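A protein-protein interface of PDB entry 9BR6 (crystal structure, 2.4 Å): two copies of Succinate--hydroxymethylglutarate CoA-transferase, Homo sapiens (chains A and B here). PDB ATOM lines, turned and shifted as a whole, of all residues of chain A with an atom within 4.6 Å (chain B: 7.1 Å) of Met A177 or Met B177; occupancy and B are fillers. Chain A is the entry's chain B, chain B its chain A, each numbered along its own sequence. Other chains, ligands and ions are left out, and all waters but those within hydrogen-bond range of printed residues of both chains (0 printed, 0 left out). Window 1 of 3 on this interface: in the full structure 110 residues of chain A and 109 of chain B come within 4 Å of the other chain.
Printed residues of chain B within 4 Å of Met A177: Met B177 (3.9 Å) and Gln B214 (3.5 Å). Of the printed residues of chain B, Leu A180 touches Cys B217. Printed residues of chain B within 4 Å of Cys A217: Val B175, Met B177 and Leu B180. Printed residues of chain A within 4 Å of Met B177: Met A177 (3.9 Å), Gln A214 (3.3 Å) and Cys A217 (3.96 Å). Of the printed residues of chain A, Leu B180 touches Cys A217. The nearest printed residue of chain B that does not touch Met A177 is Cys B217 (4.01 Å).
Among the printed residues, merely in contact across the chains: Val A175 with Leu B159, Val A175 with Cys B217, Val A175 with Leu B218, Met A177 with Met B177, Leu A180 with Cys B217, Ala A181 with Leu B184, Cys A217 with Val B175, Cys A217 with Met B177 and Cys A217 with Leu B180.
Val A175 touches Cys B217, and with the chains exchanged Cys A217 touches Val B175. Met A177 touches its own counterpart, Met B177. Met A177 touches Gln B214, and with the chains exchanged Gln A214 touches Met B177. Leu A180 touches Cys B217, and with the chains exchanged Cys A217 touches Leu B180. 11 positions are printed for both chains. Of the 11 pairs that touch across the chains among the printed residues, 7 have their exchanged pair printed and touching as well.
The side-chain sulfur (SD) of Met B177 lies within hydrogen-bond range of the side-chain amide nitrogen (NE2) of Gln A214, 3.6 Å away. The side-chain sulfur (SD) of Met A177 lies within hydrogen-bond range of the side-chain amide nitrogen (NE2) of Gln B214 (3.8 Å).
The side-chain hydroxyl (OG1) of Thr A178 is in hydrogen-bond range of the side-chain amide oxygen (OE1) of Gln A214 (2.7 Å). O of Ser B213 is in hydrogen-bond range of SG of Cys B217. OE1 of Gln B214 sits at hydrogen-bond distance from OG1 of Thr B178.
Of the 11 printed residues of chain A, 6 touch a printed residue of chain B. Printed residues of chain B that touch a printed residue of chain A: Leu B159, Val B175, Met B177, Leu B180, Leu B184, Gln B214, Cys B217 and Leu B218. Hydrophobic or aromatic side chains of chain B that line the printed part of chain A: Leu B159, Val B175, Met B177, Leu B180 and Leu B184. Among the printed residues, 11 pairs touch across the chains. Among the printed residues, no Asp or Glu carboxylate lies within 4 Å of a Lys or Arg side-chain nitrogen of the other chain.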
ATOM      1  N   ASP A 150     -15.462   1.894   7.981  1.00  0.00           N
ATOM      2  CA  ASP A 150     -15.679   0.454   7.913  1.00  0.00           C
ATOM      3  C   ASP A 150     -15.582  -0.194   9.287  1.00  0.00           C
ATOM      4  O   ASP A 150     -16.455  -0.976   9.679  1.00  0.00           O
ATOM      5  CB  ASP A 150     -14.667  -0.186   6.965  1.00  0.00           C
ATOM      6  CG  ASP A 150     -14.767  -1.697   6.955  1.00  0.00           C
ATOM      7  OD1 ASP A 150     -15.660  -2.227   6.263  1.00  0.00           O
ATOM      8  OD2 ASP A 150     -13.968  -2.356   7.660  1.00  0.00           O
ATOM      9  N   PRO A 173     -12.491  -8.068  10.110  1.00  0.00           N
ATOM     10  CA  PRO A 173     -12.022  -8.722   8.884  1.00  0.00           C
ATOM     11  C   PRO A 173     -10.821  -7.982   8.319  1.00  0.00           C
ATOM     12  O   PRO A 173     -10.701  -6.761   8.452  1.00  0.00           O
ATOM     13  CB  PRO A 173     -13.230  -8.632   7.946  1.00  0.00           C
ATOM     14  CG  PRO A 173     -14.411  -8.514   8.875  1.00  0.00           C
ATOM     15  CD  PRO A 173     -13.903  -7.660  10.004  1.00  0.00           C
ATOM     16  N   VAL A 175      -9.834  -7.291   5.212  1.00  0.00           N
ATOM     17  CA  VAL A 175     -10.245  -6.272   4.265  1.00  0.00           C
ATOM     18  C   VAL A 175     -11.569  -5.690   4.737  1.00  0.00           C
ATOM     19  O   VAL A 175     -12.307  -6.295   5.519  1.00  0.00           O
ATOM     20  CB  VAL A 175     -10.361  -6.814   2.822  1.00  0.00           C
ATOM     21  CG1 VAL A 175      -8.992  -7.064   2.235  1.00  0.00           C
ATOM     22  CG2 VAL A 175     -11.197  -8.085   2.792  1.00  0.00           C
ATOM     23  N   ALA A 176     -11.888  -4.499   4.228  1.00  0.00           N
ATOM     24  CA  ALA A 176     -13.097  -3.773   4.616  1.00  0.00           C
ATOM     25  C   ALA A 176     -14.305  -4.374   3.893  1.00  0.00           C
ATOM     26  O   ALA A 176     -14.865  -3.806   2.957  1.00  0.00           O
ATOM     27  CB  ALA A 176     -12.941  -2.291   4.307  1.00  0.00           C
ATOM     28  N   MET A 177     -14.708  -5.558   4.367  1.00  0.00           N
ATOM     29  CA  MET A 177     -15.809  -6.275   3.725  1.00  0.00           C
ATOM     30  C   MET A 177     -17.122  -5.512   3.833  1.00  0.00           C
ATOM     31  O   MET A 177     -17.967  -5.612   2.937  1.00  0.00           O
ATOM     32  CB  MET A 177     -15.955  -7.680   4.315  1.00  0.00           C
ATOM     33  CG  MET A 177     -14.854  -8.649   3.905  1.00  0.00           C
ATOM     34  SD  MET A 177     -14.700  -8.878   2.115  1.00  0.00           S
ATOM     35  CE  MET A 177     -16.093  -9.949   1.754  1.00  0.00           C
ATOM     36  N   THR A 178     -17.331  -4.771   4.922  1.00  0.00           N
ATOM     37  CA  THR A 178     -18.522  -3.930   4.995  1.00  0.00           C
ATOM     38  C   THR A 178     -18.519  -2.888   3.881  1.00  0.00           C
ATOM     39  O   THR A 178     -19.540  -2.679   3.213  1.00  0.00           O
ATOM     40  CB  THR A 178     -18.622  -3.257   6.366  1.00  0.00           C
ATOM     41  OG1 THR A 178     -18.758  -4.254   7.388  1.00  0.00           O
ATOM     42  CG2 THR A 178     -19.822  -2.324   6.412  1.00  0.00           C
ATOM     43  N   ASP A 179     -17.369  -2.248   3.646  1.00  0.00           N
ATOM     44  CA  ASP A 179     -17.257  -1.283   2.553  1.00  0.00           C
ATOM     45  C   ASP A 179     -17.485  -1.955   1.207  1.00  0.00           C
ATOM     46  O   ASP A 179     -18.227  -1.444   0.359  1.00  0.00           O
ATOM     47  CB  ASP A 179     -15.877  -0.620   2.572  1.00  0.00           C
ATOM     48  CG  ASP A 179     -15.769   0.498   3.588  1.00  0.00           C
ATOM     49  OD1 ASP A 179     -16.712   0.679   4.387  1.00  0.00           O
ATOM     50  OD2 ASP A 179     -14.732   1.196   3.581  1.00  0.00           O
ATOM     51  N   LEU A 180     -16.843  -3.104   0.992  1.00  0.00           N
ATOM     52  CA  LEU A 180     -16.956  -3.798  -0.286  1.00  0.00           C
ATOM     53  C   LEU A 180     -18.373  -4.308  -0.512  1.00  0.00           C
ATOM     54  O   LEU A 180     -18.892  -4.239  -1.634  1.00  0.00           O
ATOM     55  CB  LEU A 180     -15.944  -4.940  -0.337  1.00  0.00           C
ATOM     56  CG  LEU A 180     -14.493  -4.475  -0.196  1.00  0.00           C
ATOM     57  CD1 LEU A 180     -13.577  -5.660   0.017  1.00  0.00           C
ATOM     58  CD2 LEU A 180     -14.053  -3.672  -1.418  1.00  0.00           C
ATOM     59  N   ALA A 181     -19.017  -4.819   0.543  1.00  0.00           N
ATOM     60  CA  ALA A 181     -20.401  -5.269   0.421  1.00  0.00           C
ATOM     61  C   ALA A 181     -21.329  -4.118   0.050  1.00  0.00           C
ATOM     62  O   ALA A 181     -22.214  -4.277  -0.799  1.00  0.00           O
ATOM     63  CB  ALA A 181     -20.861  -5.930   1.721  1.00  0.00           C
ATOM     64  N   GLN A 214     -24.315  -4.258   6.225  1.00  0.00           N
ATOM     65  CA  GLN A 214     -23.774  -5.254   7.145  1.00  0.00           C
ATOM     66  C   GLN A 214     -24.881  -5.959   7.920  1.00  0.00           C
ATOM     67  O   GLN A 214     -24.814  -7.176   8.135  1.00  0.00           O
ATOM     68  CB  GLN A 214     -22.767  -4.613   8.096  1.00  0.00           C
ATOM     69  CG  GLN A 214     -21.884  -5.631   8.820  1.00  0.00           C
ATOM     70  CD  GLN A 214     -21.270  -6.669   7.885  1.00  0.00           C
ATOM     71  OE1 GLN A 214     -20.440  -6.342   7.026  1.00  0.00           O
ATOM     72  NE2 GLN A 214     -21.678  -7.927   8.049  1.00  0.00           N
ATOM     73  N   CYS A 217     -26.467  -8.545   5.843  1.00  0.00           N
ATOM     74  CA  CYS A 217     -25.584  -9.699   5.723  1.00  0.00           C
ATOM     75  C   CYS A 217     -25.614 -10.593   6.955  1.00  0.00           C
ATOM     76  O   CYS A 217     -25.265 -11.773   6.848  1.00  0.00           O
ATOM     77  CB  CYS A 217     -24.146  -9.247   5.450  1.00  0.00           C
ATOM     78  SG  CYS A 217     -23.853  -8.665   3.760  1.00  0.00           S
ATOM     79  N   LEU B  27     -26.460 -20.776   0.853  1.00  0.00           N
ATOM     80  CA  LEU B  27     -26.496 -19.349   1.151  1.00  0.00           C
ATOM     81  C   LEU B  27     -26.188 -18.456  -0.041  1.00  0.00           C
ATOM     82  O   LEU B  27     -26.921 -17.488  -0.274  1.00  0.00           O
ATOM     83  CB  LEU B  27     -25.531 -19.041   2.307  1.00  0.00           C
ATOM     84  CG  LEU B  27     -25.454 -17.586   2.761  1.00  0.00           C
ATOM     85  CD1 LEU B  27     -26.829 -17.074   3.177  1.00  0.00           C
ATOM     86  CD2 LEU B  27     -24.478 -17.464   3.915  1.00  0.00           C
ATOM     87  N   ASP B 150     -17.763 -21.732   2.449  1.00  0.00           N
ATOM     88  CA  ASP B 150     -17.308 -20.399   2.843  1.00  0.00           C
ATOM     89  C   ASP B 150     -16.001 -20.451   3.625  1.00  0.00           C
ATOM     90  O   ASP B 150     -15.060 -19.705   3.330  1.00  0.00           O
ATOM     91  CB  ASP B 150     -18.382 -19.707   3.678  1.00  0.00           C
ATOM     92  CG  ASP B 150     -17.902 -18.391   4.254  1.00  0.00           C
ATOM     93  OD1 ASP B 150     -17.895 -17.384   3.518  1.00  0.00           O
ATOM     94  OD2 ASP B 150     -17.522 -18.365   5.446  1.00  0.00           O
ATOM     95  N   LEU B 159      -8.278 -14.492   2.840  1.00  0.00           N
ATOM     96  CA  LEU B 159      -8.977 -13.638   3.793  1.00  0.00           C
ATOM     97  C   LEU B 159      -8.734 -14.095   5.225  1.00  0.00           C
ATOM     98  O   LEU B 159      -8.554 -13.267   6.126  1.00  0.00           O
ATOM     99  CB  LEU B 159     -10.474 -13.627   3.487  1.00  0.00           C
ATOM    100  CG  LEU B 159     -11.369 -12.973   4.538  1.00  0.00           C
ATOM    101  CD1 LEU B 159     -10.984 -11.513   4.729  1.00  0.00           C
ATOM    102  CD2 LEU B 159     -12.841 -13.110   4.161  1.00  0.00           C
ATOM    103  N   ARG B 172     -12.071 -16.594  11.306  1.00  0.00           N
ATOM    104  CA  ARG B 172     -12.954 -16.339  10.179  1.00  0.00           C
ATOM    105  C   ARG B 172     -14.044 -15.350  10.574  1.00  0.00           C
ATOM    106  O   ARG B 172     -14.389 -15.224  11.755  1.00  0.00           O
ATOM    107  CB  ARG B 172     -13.607 -17.632   9.672  1.00  0.00           C
ATOM    108  CG  ARG B 172     -14.677 -18.166  10.596  1.00  0.00           C
ATOM    109  CD  ARG B 172     -15.496 -19.265   9.953  1.00  0.00           C
ATOM    110  NE  ARG B 172     -16.502 -19.767  10.882  1.00  0.00           N
ATOM    111  CZ  ARG B 172     -17.740 -19.300  10.974  1.00  0.00           C
ATOM    112  NH1 ARG B 172     -18.170 -18.318  10.196  1.00  0.00           N
ATOM    113  NH2 ARG B 172     -18.568 -19.831  11.869  1.00  0.00           N
ATOM    114  N   PRO B 173     -14.611 -14.625   9.611  1.00  0.00           N
ATOM    115  CA  PRO B 173     -15.740 -13.741   9.925  1.00  0.00           C
ATOM    116  C   PRO B 173     -16.933 -14.523  10.455  1.00  0.00           C
ATOM    117  O   PRO B 173     -17.169 -15.674  10.081  1.00  0.00           O
ATOM    118  CB  PRO B 173     -16.052 -13.078   8.579  1.00  0.00           C
ATOM    119  CG  PRO B 173     -14.753 -13.147   7.833  1.00  0.00           C
ATOM    120  CD  PRO B 173     -14.164 -14.464   8.217  1.00  0.00           C
ATOM    121  N   GLY B 174     -17.692 -13.867  11.338  1.00  0.00           N
ATOM    122  CA  GLY B 174     -18.822 -14.527  11.976  1.00  0.00           C
ATOM    123  C   GLY B 174     -19.864 -15.004  10.986  1.00  0.00           C
ATOM    124  O   GLY B 174     -20.391 -16.113  11.110  1.00  0.00           O
ATOM    125  N   VAL B 175     -20.192 -14.170  10.005  1.00  0.00           N
ATOM    126  CA  VAL B 175     -21.083 -14.552   8.927  1.00  0.00           C
ATOM    127  C   VAL B 175     -20.246 -14.933   7.712  1.00  0.00           C
ATOM    128  O   VAL B 175     -19.078 -14.560   7.583  1.00  0.00           O
ATOM    129  CB  VAL B 175     -22.076 -13.418   8.584  1.00  0.00           C
ATOM    130  CG1 VAL B 175     -23.250 -13.950   7.781  1.00  0.00           C
ATOM    131  CG2 VAL B 175     -22.563 -12.751   9.850  1.00  0.00           C
ATOM    132  N   ALA B 176     -20.863 -15.675   6.792  1.00  0.00           N
ATOM    133  CA  ALA B 176     -20.195 -16.138   5.577  1.00  0.00           C
ATOM    134  C   ALA B 176     -20.135 -14.988   4.567  1.00  0.00           C
ATOM    135  O   ALA B 176     -20.845 -14.950   3.562  1.00  0.00           O
ATOM    136  CB  ALA B 176     -20.919 -17.350   5.007  1.00  0.00           C
ATOM    137  N   MET B 177     -19.244 -14.036   4.856  1.00  0.00           N
ATOM    138  CA  MET B 177     -19.116 -12.851   4.007  1.00  0.00           C
ATOM    139  C   MET B 177     -18.641 -13.208   2.602  1.00  0.00           C
ATOM    140  O   MET B 177     -18.985 -12.514   1.639  1.00  0.00           O
ATOM    141  CB  MET B 177     -18.178 -11.829   4.654  1.00  0.00           C
ATOM    142  CG  MET B 177     -18.773 -11.112   5.870  1.00  0.00           C
ATOM    143  SD  MET B 177     -20.295 -10.173   5.564  1.00  0.00           S
ATOM    144  CE  MET B 177     -19.661  -8.689   4.783  1.00  0.00           C
ATOM    145  N   THR B 178     -17.820 -14.251   2.462  1.00  0.00           N
ATOM    146  CA  THR B 178     -17.438 -14.699   1.124  1.00  0.00           C
ATOM    147  C   THR B 178     -18.650 -15.166   0.321  1.00  0.00           C
ATOM    148  O   THR B 178     -18.789 -14.819  -0.858  1.00  0.00           O
ATOM    149  CB  THR B 178     -16.392 -15.814   1.205  1.00  0.00           C
ATOM    150  OG1 THR B 178     -15.188 -15.306   1.795  1.00  0.00           O
ATOM    151  CG2 THR B 178     -16.093 -16.368  -0.177  1.00  0.00           C
ATOM    152  N   ASP B 179     -19.538 -15.948   0.942  1.00  0.00           N
ATOM    153  CA  ASP B 179     -20.742 -16.399   0.246  1.00  0.00           C
ATOM    154  C   ASP B 179     -21.628 -15.220  -0.127  1.00  0.00           C
ATOM    155  O   ASP B 179     -22.104 -15.118  -1.264  1.00  0.00           O
ATOM    156  CB  ASP B 179     -21.524 -17.385   1.118  1.00  0.00           C
ATOM    157  CG  ASP B 179     -20.963 -18.793   1.070  1.00  0.00           C
ATOM    158  OD1 ASP B 179     -19.879 -18.989   0.483  1.00  0.00           O
ATOM    159  OD2 ASP B 179     -21.620 -19.711   1.614  1.00  0.00           O
ATOM    160  N   LEU B 180     -21.855 -14.315   0.826  1.00  0.00           N
ATOM    161  CA  LEU B 180     -22.730 -13.175   0.593  1.00  0.00           C
ATOM    162  C   LEU B 180     -22.142 -12.241  -0.459  1.00  0.00           C
ATOM    163  O   LEU B 180     -22.879 -11.678  -1.279  1.00  0.00           O
ATOM    164  CB  LEU B 180     -22.972 -12.443   1.911  1.00  0.00           C
ATOM    165  CG  LEU B 180     -23.629 -13.294   3.004  1.00  0.00           C
ATOM    166  CD1 LEU B 180     -23.549 -12.569   4.321  1.00  0.00           C
ATOM    167  CD2 LEU B 180     -25.085 -13.632   2.678  1.00  0.00           C
ATOM    168  N   ALA B 181     -20.819 -12.060  -0.448  1.00  0.00           N
ATOM    169  CA  ALA B 181     -20.188 -11.244  -1.480  1.00  0.00           C
ATOM    170  C   ALA B 181     -20.416 -11.844  -2.857  1.00  0.00           C
ATOM    171  O   ALA B 181     -20.776 -11.130  -3.801  1.00  0.00           O
ATOM    172  CB  ALA B 181     -18.691 -11.102  -1.205  1.00  0.00           C
ATOM    173  N   THR B 182     -20.253 -13.162  -2.981  1.00  0.00           N
ATOM    174  CA  THR B 182     -20.518 -13.818  -4.256  1.00  0.00           C
ATOM    175  C   THR B 182     -21.979 -13.659  -4.659  1.00  0.00           C
ATOM    176  O   THR B 182     -22.285 -13.413  -5.833  1.00  0.00           O
ATOM    177  CB  THR B 182     -20.142 -15.298  -4.171  1.00  0.00           C
ATOM    178  OG1 THR B 182     -18.781 -15.423  -3.737  1.00  0.00           O
ATOM    179  CG2 THR B 182     -20.283 -15.957  -5.534  1.00  0.00           C
ATOM    180  N   GLY B 183     -22.896 -13.783  -3.697  1.00  0.00           N
ATOM    181  CA  GLY B 183     -24.303 -13.573  -4.000  1.00  0.00           C
ATOM    182  C   GLY B 183     -24.593 -12.160  -4.471  1.00  0.00           C
ATOM    183  O   GLY B 183     -25.391 -11.956  -5.389  1.00  0.00           O
ATOM    184  N   LEU B 184     -23.953 -11.168  -3.845  1.00  0.00           N
ATOM    185  CA  LEU B 184     -24.115  -9.787  -4.293  1.00  0.00           C
ATOM    186  C   LEU B 184     -23.536  -9.593  -5.692  1.00  0.00           C
ATOM    187  O   LEU B 184     -24.103  -8.855  -6.509  1.00  0.00           O
ATOM    188  CB  LEU B 184     -23.467  -8.830  -3.288  1.00  0.00           C
ATOM    189  CG  LEU B 184     -24.161  -8.692  -1.922  1.00  0.00           C
ATOM    190  CD1 LEU B 184     -23.449  -7.681  -1.029  1.00  0.00           C
ATOM    191  CD2 LEU B 184     -25.626  -8.302  -2.085  1.00  0.00           C
ATOM    192  N   SER B 213     -14.606 -13.960  -6.100  1.00  0.00           N
ATOM    193  CA  SER B 213     -15.192 -12.850  -5.353  1.00  0.00           C
ATOM    194  C   SER B 213     -14.283 -12.418  -4.210  1.00  0.00           C
ATOM    195  O   SER B 213     -13.993 -11.227  -4.047  1.00  0.00           O
ATOM    196  CB  SER B 213     -16.566 -13.241  -4.810  1.00  0.00           C
ATOM    197  OG  SER B 213     -17.455 -13.598  -5.851  1.00  0.00           O
ATOM    198  N   GLN B 214     -13.809 -13.378  -3.415  1.00  0.00           N
ATOM    199  CA  GLN B 214     -12.997 -13.027  -2.256  1.00  0.00           C
ATOM    200  C   GLN B 214     -11.645 -12.464  -2.674  1.00  0.00           C
ATOM    201  O   GLN B 214     -11.158 -11.499  -2.071  1.00  0.00           O
ATOM    202  CB  GLN B 214     -12.827 -14.236  -1.337  1.00  0.00           C
ATOM    203  CG  GLN B 214     -12.307 -13.858   0.037  1.00  0.00           C
ATOM    204  CD  GLN B 214     -13.062 -12.697   0.655  1.00  0.00           C
ATOM    205  OE1 GLN B 214     -14.249 -12.807   0.976  1.00  0.00           O
ATOM    206  NE2 GLN B 214     -12.379 -11.566   0.813  1.00  0.00           N
ATOM    207  N   CYS B 217     -12.024  -8.980  -3.746  1.00  0.00           N
ATOM    208  CA  CYS B 217     -12.226  -8.140  -2.571  1.00  0.00           C
ATOM    209  C   CYS B 217     -10.924  -7.833  -1.833  1.00  0.00           C
ATOM    210  O   CYS B 217     -10.868  -6.840  -1.100  1.00  0.00           O
ATOM    211  CB  CYS B 217     -13.228  -8.797  -1.618  1.00  0.00           C
ATOM    212  SG  CYS B 217     -14.963  -8.693  -2.171  1.00  0.00           S
ATOM    213  N   LEU B 218      -9.883  -8.657  -1.998  1.00  0.00           N
ATOM    214  CA  LEU B 218      -8.605  -8.366  -1.351  1.00  0.00           C
ATOM    215  C   LEU B 218      -8.077  -6.999  -1.768  1.00  0.00           C
ATOM    216  O   LEU B 218      -7.427  -6.308  -0.975  1.00  0.00           O
ATOM    217  CB  LEU B 218      -7.581  -9.454  -1.668  1.00  0.00           C
ATOM    218  CG  LEU B 218      -7.855 -10.823  -1.049  1.00  0.00           C
ATOM    219  CD1 LEU B 218      -6.747 -11.787  -1.429  1.00  0.00           C
ATOM    220  CD2 LEU B 218      -8.030 -10.739   0.468  1.00  0.00           C
